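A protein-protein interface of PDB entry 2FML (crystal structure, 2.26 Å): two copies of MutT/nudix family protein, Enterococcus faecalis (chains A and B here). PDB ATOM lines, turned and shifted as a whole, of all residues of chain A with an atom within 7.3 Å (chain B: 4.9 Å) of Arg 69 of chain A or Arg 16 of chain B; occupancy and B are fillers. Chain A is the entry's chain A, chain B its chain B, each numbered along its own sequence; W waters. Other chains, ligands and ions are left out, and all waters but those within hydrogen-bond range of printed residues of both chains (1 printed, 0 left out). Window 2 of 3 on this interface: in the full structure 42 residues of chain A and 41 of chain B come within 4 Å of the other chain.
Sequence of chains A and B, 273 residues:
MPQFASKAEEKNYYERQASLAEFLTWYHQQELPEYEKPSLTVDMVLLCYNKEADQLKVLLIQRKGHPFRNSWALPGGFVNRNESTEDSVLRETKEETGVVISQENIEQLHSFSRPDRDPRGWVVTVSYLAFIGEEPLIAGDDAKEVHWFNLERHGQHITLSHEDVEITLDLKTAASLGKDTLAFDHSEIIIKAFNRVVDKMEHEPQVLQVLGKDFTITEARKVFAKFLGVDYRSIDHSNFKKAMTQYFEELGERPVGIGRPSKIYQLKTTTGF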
ATOM      1  N   GLN A  62     -27.797  30.797 -15.713  1.00  0.00           N
ATOM      2  CA  GLN A  62     -28.861  29.836 -15.977  1.00  0.00           C
ATOM      3  C   GLN A  62     -28.217  28.469 -16.011  1.00  0.00           C
ATOM      4  O   GLN A  62     -27.364  28.185 -16.858  1.00  0.00           O
ATOM      5  CB  GLN A  62     -29.614  30.103 -17.282  1.00  0.00           C
ATOM      6  CG  GLN A  62     -30.710  29.093 -17.504  1.00  0.00           C
ATOM      7  CD  GLN A  62     -31.574  29.367 -18.711  1.00  0.00           C
ATOM      8  OE1 GLN A  62     -32.824  29.281 -18.646  1.00  0.00           O
ATOM      9  NE2 GLN A  62     -30.939  29.664 -19.817  1.00  0.00           N
ATOM     10  N   ARG A  63     -28.644  27.627 -15.075  1.00  0.00           N
ATOM     11  CA  ARG A  63     -28.082  26.281 -14.936  1.00  0.00           C
ATOM     12  C   ARG A  63     -28.444  25.431 -16.124  1.00  0.00           C
ATOM     13  O   ARG A  63     -29.570  25.431 -16.578  1.00  0.00           O
ATOM     14  CB  ARG A  63     -28.593  25.647 -13.652  1.00  0.00           C
ATOM     15  CG  ARG A  63     -28.244  26.502 -12.364  1.00  0.00           C
ATOM     16  CD  ARG A  63     -28.754  25.781 -11.124  1.00  0.00           C
ATOM     17  NE  ARG A  63     -28.467  24.345 -11.157  1.00  0.00           N
ATOM     18  CZ  ARG A  63     -27.326  23.774 -10.769  1.00  0.00           C
ATOM     19  NH1 ARG A  63     -26.302  24.519 -10.301  1.00  0.00           N
ATOM     20  NH2 ARG A  63     -27.210  22.444 -10.875  1.00  0.00           N
ATOM     21  N   LYS A  64     -27.497  24.688 -16.642  1.00  0.00           N
ATOM     22  CA  LYS A  64     -27.843  23.887 -17.762  1.00  0.00           C
ATOM     23  C   LYS A  64     -28.168  22.425 -17.408  1.00  0.00           C
ATOM     24  O   LYS A  64     -28.821  21.737 -18.168  1.00  0.00           O
ATOM     25  CB  LYS A  64     -26.798  24.047 -18.865  1.00  0.00           C
ATOM     26  CG  LYS A  64     -25.623  23.139 -18.889  1.00  0.00           C
ATOM     27  CD  LYS A  64     -25.218  22.974 -20.420  1.00  0.00           C
ATOM     28  CE  LYS A  64     -24.822  24.323 -21.113  1.00  0.00           C
ATOM     29  NZ  LYS A  64     -23.687  24.176 -22.133  1.00  0.00           N
ATOM     30  N   GLY A  65     -27.753  22.006 -16.217  1.00  0.00           N
ATOM     31  CA  GLY A  65     -27.961  20.662 -15.739  1.00  0.00           C
ATOM     32  C   GLY A  65     -28.715  20.640 -14.435  1.00  0.00           C
ATOM     33  O   GLY A  65     -28.814  21.684 -13.718  1.00  0.00           O
ATOM     34  N   HIS A  66     -29.249  19.453 -14.137  1.00  0.00           N
ATOM     35  CA  HIS A  66     -29.948  19.196 -12.908  1.00  0.00           C
ATOM     36  C   HIS A  66     -29.016  19.216 -11.687  1.00  0.00           C
ATOM     37  O   HIS A  66     -27.835  18.973 -11.815  1.00  0.00           O
ATOM     38  CB  HIS A  66     -30.705  17.870 -13.022  1.00  0.00           C
ATOM     39  CG  HIS A  66     -32.084  18.019 -13.578  1.00  0.00           C
ATOM     40  ND1 HIS A  66     -32.681  17.066 -14.376  1.00  0.00           N
ATOM     41  CD2 HIS A  66     -32.985  19.015 -13.443  1.00  0.00           C
ATOM     42  CE1 HIS A  66     -33.886  17.477 -14.716  1.00  0.00           C
ATOM     43  NE2 HIS A  66     -34.082  18.671 -14.187  1.00  0.00           N
ATOM     44  N   PRO A  67     -29.555  19.460 -10.474  1.00  0.00           N
ATOM     45  CA  PRO A  67     -30.910  19.854 -10.109  1.00  0.00           C
ATOM     46  C   PRO A  67     -31.159  21.301 -10.524  1.00  0.00           C
ATOM     47  O   PRO A  67     -30.204  22.042 -10.766  1.00  0.00           O
ATOM     48  CB  PRO A  67     -30.949  19.649  -8.591  1.00  0.00           C
ATOM     49  CG  PRO A  67     -29.511  19.633  -8.132  1.00  0.00           C
ATOM     50  CD  PRO A  67     -28.686  19.229  -9.310  1.00  0.00           C
ATOM     51  N   PHE A  68     -32.421  21.666 -10.739  1.00  0.00           N
ATOM     52  CA  PHE A  68     -32.794  23.002 -11.176  1.00  0.00           C
ATOM     53  C   PHE A  68     -32.238  23.367 -12.493  1.00  0.00           C
ATOM     54  O   PHE A  68     -31.800  24.513 -12.650  1.00  0.00           O
ATOM     55  CB  PHE A  68     -32.353  24.049 -10.108  1.00  0.00           C
ATOM     56  CG  PHE A  68     -33.022  23.830  -8.760  1.00  0.00           C
ATOM     57  CD1 PHE A  68     -34.373  24.201  -8.563  1.00  0.00           C
ATOM     58  CD2 PHE A  68     -32.339  23.202  -7.719  1.00  0.00           C
ATOM     59  CE1 PHE A  68     -35.013  23.986  -7.309  1.00  0.00           C
ATOM     60  CE2 PHE A  68     -32.968  22.975  -6.479  1.00  0.00           C
ATOM     61  CZ  PHE A  68     -34.293  23.376  -6.277  1.00  0.00           C
ATOM     62  N   ARG A  69     -32.253  22.416 -13.448  1.00  0.00           N
ATOM     63  CA  ARG A  69     -32.001  22.716 -14.837  1.00  0.00           C
ATOM     64  C   ARG A  69     -32.829  23.905 -15.340  1.00  0.00           C
ATOM     65  O   ARG A  69     -34.037  23.947 -15.154  1.00  0.00           O
ATOM     66  CB  ARG A  69     -32.320  21.512 -15.721  1.00  0.00           C
ATOM     67  CG  ARG A  69     -31.897  21.649 -17.165  1.00  0.00           C
ATOM     68  CD  ARG A  69     -32.608  20.587 -18.026  1.00  0.00           C
ATOM     69  NE  ARG A  69     -32.229  19.253 -17.593  1.00  0.00           N
ATOM     70  CZ  ARG A  69     -32.902  18.114 -17.799  1.00  0.00           C
ATOM     71  NH1 ARG A  69     -34.091  18.076 -18.399  1.00  0.00           N
ATOM     72  NH2 ARG A  69     -32.365  16.987 -17.323  1.00  0.00           N
ATOM     73  N   ASN A  70     -32.154  24.853 -15.991  1.00  0.00           N
ATOM     74  CA  ASN A  70     -32.811  26.005 -16.588  1.00  0.00           C
ATOM     75  C   ASN A  70     -33.260  27.096 -15.610  1.00  0.00           C
ATOM     76  O   ASN A  70     -33.773  28.137 -16.011  1.00  0.00           O
ATOM     77  CB  ASN A  70     -33.970  25.543 -17.507  1.00  0.00           C
ATOM     78  CG  ASN A  70     -33.471  24.828 -18.773  1.00  0.00           C
ATOM     79  OD1 ASN A  70     -32.314  24.951 -19.161  1.00  0.00           O
ATOM     80  ND2 ASN A  70     -34.359  24.072 -19.413  1.00  0.00           N
ATOM     81  N   SER A  71     -33.064  26.869 -14.324  1.00  0.00           N
ATOM     82  CA  SER A  71     -33.342  27.884 -13.341  1.00  0.00           C
ATOM     83  C   SER A  71     -32.127  28.841 -13.310  1.00  0.00           C
ATOM     84  O   SER A  71     -31.024  28.432 -13.612  1.00  0.00           O
ATOM     85  CB  SER A  71     -33.586  27.252 -11.961  1.00  0.00           C
ATOM     86  OG  SER A  71     -34.783  26.506 -11.934  1.00  0.00           O
ATOM     87  N   TRP A  72     -32.356  30.085 -12.908  1.00  0.00           N
ATOM     88  CA  TRP A  72     -31.295  31.025 -12.607  1.00  0.00           C
ATOM     89  C   TRP A  72     -30.791  30.806 -11.180  1.00  0.00           C
ATOM     90  O   TRP A  72     -31.527  30.374 -10.294  1.00  0.00           O
ATOM     91  CB  TRP A  72     -31.745  32.495 -12.848  1.00  0.00           C
ATOM     92  CG  TRP A  72     -32.161  32.720 -14.266  1.00  0.00           C
ATOM     93  CD1 TRP A  72     -33.435  32.574 -14.778  1.00  0.00           C
ATOM     94  CD2 TRP A  72     -31.319  33.081 -15.383  1.00  0.00           C
ATOM     95  NE1 TRP A  72     -33.428  32.824 -16.127  1.00  0.00           N
ATOM     96  CE2 TRP A  72     -32.155  33.160 -16.523  1.00  0.00           C
ATOM     97  CE3 TRP A  72     -29.945  33.358 -15.529  1.00  0.00           C
ATOM     98  CZ2 TRP A  72     -31.658  33.490 -17.803  1.00  0.00           C
ATOM     99  CZ3 TRP A  72     -29.460  33.701 -16.794  1.00  0.00           C
ATOM    100  CH2 TRP A  72     -30.313  33.779 -17.910  1.00  0.00           C
ATOM    101  N   GLY A 140     -19.190  29.224 -18.468  1.00  0.00           N
ATOM    102  CA  GLY A 140     -18.483  27.961 -18.449  1.00  0.00           C
ATOM    103  C   GLY A 140     -19.473  26.972 -19.020  1.00  0.00           C
ATOM    104  O   GLY A 140     -20.595  27.349 -19.398  1.00  0.00           O
ATOM    105  N   ASP A 141     -19.073  25.706 -19.059  1.00  0.00           N
ATOM    106  CA  ASP A 141     -19.847  24.640 -19.702  1.00  0.00           C
ATOM    107  C   ASP A 141     -21.213  24.386 -19.062  1.00  0.00           C
ATOM    108  O   ASP A 141     -22.183  24.106 -19.785  1.00  0.00           O
ATOM    109  CB  ASP A 141     -19.051  23.336 -19.712  1.00  0.00           C
ATOM    110  CG  ASP A 141     -19.669  22.283 -20.634  1.00  0.00           C
ATOM    111  OD1 ASP A 141     -20.094  22.635 -21.770  1.00  0.00           O
ATOM    112  OD2 ASP A 141     -19.728  21.101 -20.213  1.00  0.00           O
ATOM    113  N   ASP A 142     -21.265  24.477 -17.731  1.00  0.00           N
ATOM    114  CA  ASP A 142     -22.516  24.277 -16.920  1.00  0.00           C
ATOM    115  C   ASP A 142     -23.474  25.479 -16.838  1.00  0.00           C
ATOM    116  O   ASP A 142     -24.506  25.426 -16.166  1.00  0.00           O
ATOM    117  CB  ASP A 142     -22.190  23.771 -15.506  1.00  0.00           C
ATOM    118  CG  ASP A 142     -21.373  22.470 -15.523  1.00  0.00           C
ATOM    119  OD1 ASP A 142     -21.593  21.592 -16.415  1.00  0.00           O
ATOM    120  OD2 ASP A 142     -20.507  22.323 -14.628  1.00  0.00           O
ATOM    121  N   ALA A 143     -23.145  26.542 -17.554  1.00  0.00           N
ATOM    122  CA  ALA A 143     -23.939  27.725 -17.518  1.00  0.00           C
ATOM    123  C   ALA A 143     -24.438  27.948 -18.910  1.00  0.00           C
ATOM    124  O   ALA A 143     -23.626  28.064 -19.846  1.00  0.00           O
ATOM    125  CB  ALA A 143     -23.099  28.892 -17.045  1.00  0.00           C
ATOM    126  N   LYS A 144     -25.762  27.965 -19.055  1.00  0.00           N
ATOM    127  CA  LYS A 144     -26.434  28.174 -20.354  1.00  0.00           C
ATOM    128  C   LYS A 144     -26.407  29.657 -20.701  1.00  0.00           C
ATOM    129  O   LYS A 144     -26.424  30.045 -21.844  1.00  0.00           O
ATOM    130  CB  LYS A 144     -27.902  27.743 -20.268  1.00  0.00           C
ATOM    131  CG  LYS A 144     -28.298  26.529 -21.049  1.00  0.00           C
ATOM    132  CD  LYS A 144     -29.820  26.382 -21.017  1.00  0.00           C
ATOM    133  CE  LYS A 144     -30.504  26.919 -22.268  1.00  0.00           C
ATOM    134  NZ  LYS A 144     -31.860  26.290 -22.423  1.00  0.00           N
ATOM    135  N   ALA A 183     -32.973  28.938  -8.207  1.00  0.00           N
ATOM    136  CA  ALA A 183     -32.553  27.609  -7.798  1.00  0.00           C
ATOM    137  C   ALA A 183     -32.188  27.482  -6.301  1.00  0.00           C
ATOM    138  O   ALA A 183     -31.710  28.420  -5.659  1.00  0.00           O
ATOM    139  CB  ALA A 183     -31.350  27.142  -8.683  1.00  0.00           C
ATOM    140  N   ASN B  12     -23.723  13.390 -18.995  1.00  0.00           N
ATOM    141  CA  ASN B  12     -24.426  14.407 -19.778  1.00  0.00           C
ATOM    142  C   ASN B  12     -25.908  14.109 -20.011  1.00  0.00           C
ATOM    143  O   ASN B  12     -26.758  15.009 -19.846  1.00  0.00           O
ATOM    144  CB  ASN B  12     -23.719  14.636 -21.117  1.00  0.00           C
ATOM    145  CG  ASN B  12     -24.206  15.890 -21.822  1.00  0.00           C
ATOM    146  OD1 ASN B  12     -25.328  15.920 -22.429  1.00  0.00           O
ATOM    147  ND2 ASN B  12     -23.375  16.952 -21.740  1.00  0.00           N
ATOM    148  N   TYR B  13     -26.241  12.865 -20.390  1.00  0.00           N
ATOM    149  CA  TYR B  13     -27.678  12.563 -20.480  1.00  0.00           C
ATOM    150  C   TYR B  13     -28.512  12.843 -19.179  1.00  0.00           C
ATOM    151  O   TYR B  13     -29.622  13.371 -19.241  1.00  0.00           O
ATOM    152  CB  TYR B  13     -27.898  11.138 -20.925  1.00  0.00           C
ATOM    153  CG  TYR B  13     -29.342  10.712 -20.842  1.00  0.00           C
ATOM    154  CD1 TYR B  13     -29.818  10.088 -19.705  1.00  0.00           C
ATOM    155  CD2 TYR B  13     -30.224  10.903 -21.929  1.00  0.00           C
ATOM    156  CE1 TYR B  13     -31.166   9.722 -19.599  1.00  0.00           C
ATOM    157  CE2 TYR B  13     -31.558  10.514 -21.850  1.00  0.00           C
ATOM    158  CZ  TYR B  13     -32.018   9.922 -20.682  1.00  0.00           C
ATOM    159  OH  TYR B  13     -33.349   9.524 -20.553  1.00  0.00           O
ATOM    160  N   TYR B  14     -27.986  12.434 -18.022  1.00  0.00           N
ATOM    161  CA  TYR B  14     -28.753  12.499 -16.771  1.00  0.00           C
ATOM    162  C   TYR B  14     -28.915  13.909 -16.270  1.00  0.00           C
ATOM    163  O   TYR B  14     -29.957  14.256 -15.782  1.00  0.00           O
ATOM    164  CB  TYR B  14     -28.139  11.599 -15.683  1.00  0.00           C
ATOM    165  CG  TYR B  14     -28.439  10.165 -15.968  1.00  0.00           C
ATOM    166  CD1 TYR B  14     -27.464   9.275 -16.496  1.00  0.00           C
ATOM    167  CD2 TYR B  14     -29.750   9.704 -15.803  1.00  0.00           C
ATOM    168  CE1 TYR B  14     -27.825   7.921 -16.804  1.00  0.00           C
ATOM    169  CE2 TYR B  14     -30.092   8.399 -16.091  1.00  0.00           C
ATOM    170  CZ  TYR B  14     -29.158   7.519 -16.577  1.00  0.00           C
ATOM    171  OH  TYR B  14     -29.686   6.274 -16.812  1.00  0.00           O
ATOM    172  N   GLU B  15     -27.862  14.699 -16.369  1.00  0.00           N
ATOM    173  CA  GLU B  15     -27.895  16.121 -15.996  1.00  0.00           C
ATOM    174  C   GLU B  15     -28.773  16.993 -16.914  1.00  0.00           C
ATOM    175  O   GLU B  15     -29.449  17.903 -16.424  1.00  0.00           O
ATOM    176  CB  GLU B  15     -26.472  16.681 -15.917  1.00  0.00           C
ATOM    177  CG  GLU B  15     -25.655  16.001 -14.827  1.00  0.00           C
ATOM    178  CD  GLU B  15     -24.242  16.594 -14.574  1.00  0.00           C
ATOM    179  OE1 GLU B  15     -23.578  17.064 -15.519  1.00  0.00           O
ATOM    180  OE2 GLU B  15     -23.790  16.572 -13.393  1.00  0.00           O
ATOM    181  N   ARG B  16     -28.747  16.714 -18.231  1.00  0.00           N
ATOM    182  CA  ARG B  16     -29.180  17.683 -19.251  1.00  0.00           C
ATOM    183  C   ARG B  16     -30.448  17.283 -20.036  1.00  0.00           C
ATOM    184  O   ARG B  16     -31.176  18.150 -20.578  1.00  0.00           O
ATOM    185  CB  ARG B  16     -28.003  18.019 -20.191  1.00  0.00           C
ATOM    186  CG  ARG B  16     -26.728  18.465 -19.460  1.00  0.00           C
ATOM    187  CD  ARG B  16     -25.761  19.155 -20.401  1.00  0.00           C
ATOM    188  NE  ARG B  16     -24.556  19.661 -19.725  1.00  0.00           N
ATOM    189  CZ  ARG B  16     -23.501  20.133 -20.376  1.00  0.00           C
ATOM    190  NH1 ARG B  16     -23.514  20.169 -21.696  1.00  0.00           N
ATOM    191  NH2 ARG B  16     -22.452  20.591 -19.713  1.00  0.00           N
ATOM    192  N   GLN B  17     -30.706  15.977 -20.098  1.00  0.00           N
ATOM    193  CA  GLN B  17     -31.852  15.476 -20.812  1.00  0.00           C
ATOM    194  C   GLN B  17     -32.845  14.730 -19.942  1.00  0.00           C
ATOM    195  O   GLN B  17     -34.013  14.720 -20.253  1.00  0.00           O
ATOM    196  CB  GLN B  17     -31.400  14.569 -21.984  1.00  0.00           C
ATOM    197  CG  GLN B  17     -30.391  15.192 -22.952  1.00  0.00           C
ATOM    198  CD  GLN B  17     -29.971  14.181 -24.011  1.00  0.00           C
ATOM    199  OE1 GLN B  17     -30.799  13.365 -24.465  1.00  0.00           O
ATOM    200  NE2 GLN B  17     -28.683  14.209 -24.411  1.00  0.00           N
ATOM    201  N   ALA B  18     -32.412  14.088 -18.863  1.00  0.00           N
ATOM    202  CA  ALA B  18     -33.314  13.225 -18.123  1.00  0.00           C
ATOM    203  C   ALA B  18     -34.227  14.082 -17.211  1.00  0.00           C
ATOM    204  O   ALA B  18     -33.970  15.257 -16.992  1.00  0.00           O
ATOM    205  CB  ALA B  18     -32.531  12.195 -17.286  1.00  0.00           C
ATOM    206  N   SER B  19     -35.290  13.478 -16.730  1.00  0.00           N
ATOM    207  CA  SER B  19     -36.156  14.097 -15.724  1.00  0.00           C
ATOM    208  C   SER B  19     -35.400  14.232 -14.392  1.00  0.00           C
ATOM    209  O   SER B  19     -34.332  13.566 -14.192  1.00  0.00           O
ATOM    210  CB  SER B  19     -37.397  13.241 -15.562  1.00  0.00           C
ATOM    211  OG  SER B  19     -37.089  12.117 -14.780  1.00  0.00           O
HETATM  212  O   HOH W   1     -24.431  19.958 -16.622  1.00  0.00           O
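Of the printed residues of chain B, Lys 64 of chain A touches Arg 16 (3.3 Å).
Arg 69 of chain A touches five residues of chain B.
Ser 71 of chain A touches none of the printed residues of chain B.
Printed residues of chain B within 4 Å of Asp 142 of chain A: Arg 16 (3.6 Å).
Lys 144 of chain A touches none of the printed residues of chain B.
Of the printed residues of chain A, Glu 15 of chain B touches Gly 65 (3.2 Å), His 66 (2.8 Å) and Arg 69 (3.2 Å).
Of the printed residues of chain A, Gln 17 of chain B touches Arg 69.
The nearest residue of chain B that does not touch Arg 69 of chain A is Ser 19 of chain B (4.6 Å).
Of the 17 printed residues of chain A, 6 touch a printed residue of chain B.
Hydrophobic or aromatic side chains of chain A that line the printed part of chain B: His 66.
Printed residues of chain B that touch a printed residue of chain A: Tyr 14, Glu 15, Arg 16, Gln 17, Ala 18 and Ser 19.
Among the printed residues, 12 pairs touch across the chains.
Among the printed residues, Asp or Glu carboxylates within 4 Å of a Lys or Arg side-chain nitrogen of the other chain: Asp 141 of chain A with Arg 16 of chain B and Asp 142 of chain A with Arg 16 of chain B.
Water W1 lies within hydrogen-bond range of NE of Arg 16 of chain B (3.1 Å), OE1 of Glu 15 of chain B (3.2 Å) and OD1 of Asp 142 of chain A (3.3 Å).
The backbone carbonyl oxygen (O) of Glu 15 of chain B sits at hydrogen-bond distance from the backbone NH (N) of His 66 of chain A (2.8 Å).
The guanidinium group (NH2) of Arg 69 of chain A lies close to the backbone NH (N) of Gln 17 of chain B.
ND1 of His 66 of chain A sits close to O of Ala 18 of chain B, at 3.4 Å.
The side-chain carboxylate (OD1) of Asp 142 of chain A lies within salt-bridge range of the guanidinium group (NH2) of Arg 16 of chain B (3.6 Å).
The guanidinium group of Arg 69 of chain A sits at hydrogen-bond distance from the backbone carbonyl oxygen of Glu 15 of chain B.
The guanidinium group (NH2) of Arg 16 of chain B lies within salt-bridge range of the side-chain carboxylate (OD2) of Asp 141 of chain A.
The backbone carbonyl oxygen (O) of Arg 16 of chain B sits close to the guanidinium group (NE) of Arg 69 of chain A (3.4 Å).
The guanidinium group of Arg 69 of chain A lies within hydrogen-bond range of the backbone carbonyl oxygen of Ala 18 of chain B, at 3.2 Å.
No position is printed for both chains.
The side-chain amino group (NZ) of Lys 64 of chain A lies within salt-bridge range of the side-chain carboxylate (OD1) of Asp 141 of chain A.
NH2 of Arg 63 of chain A lies within hydrogen-bond range of O of Gly 65 of chain A (3.4 Å).
The backbone NH (N) of Ala 18 of chain B sits at hydrogen-bond distance from the backbone carbonyl oxygen (O) of Tyr 13 of chain B.
The backbone NH of Lys 64 of chain A lies within hydrogen-bond range of the backbone carbonyl oxygen of Asp 142 of chain A (3.1 Å).
The guanidinium group (NH1) of Arg 16 of chain B sits close to the side-chain amide nitrogen (ND2) of Asn 12 of chain B.
ND1 of His 66 of chain A lies within hydrogen-bond range of NH2 of Arg 69 of chain A, at 3.0 Å.
Arg 16 of chain B touches Lys 64 of chain A.
O of Glu 15 of chain B touches CA of Gly 65 of chain A, 3.2 Å away.
His 66 of chain A touches Ser 19 of chain B.
Arg 69 of chain A touches Tyr 14 of chain B (NH2 to O, 3.95 Å).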
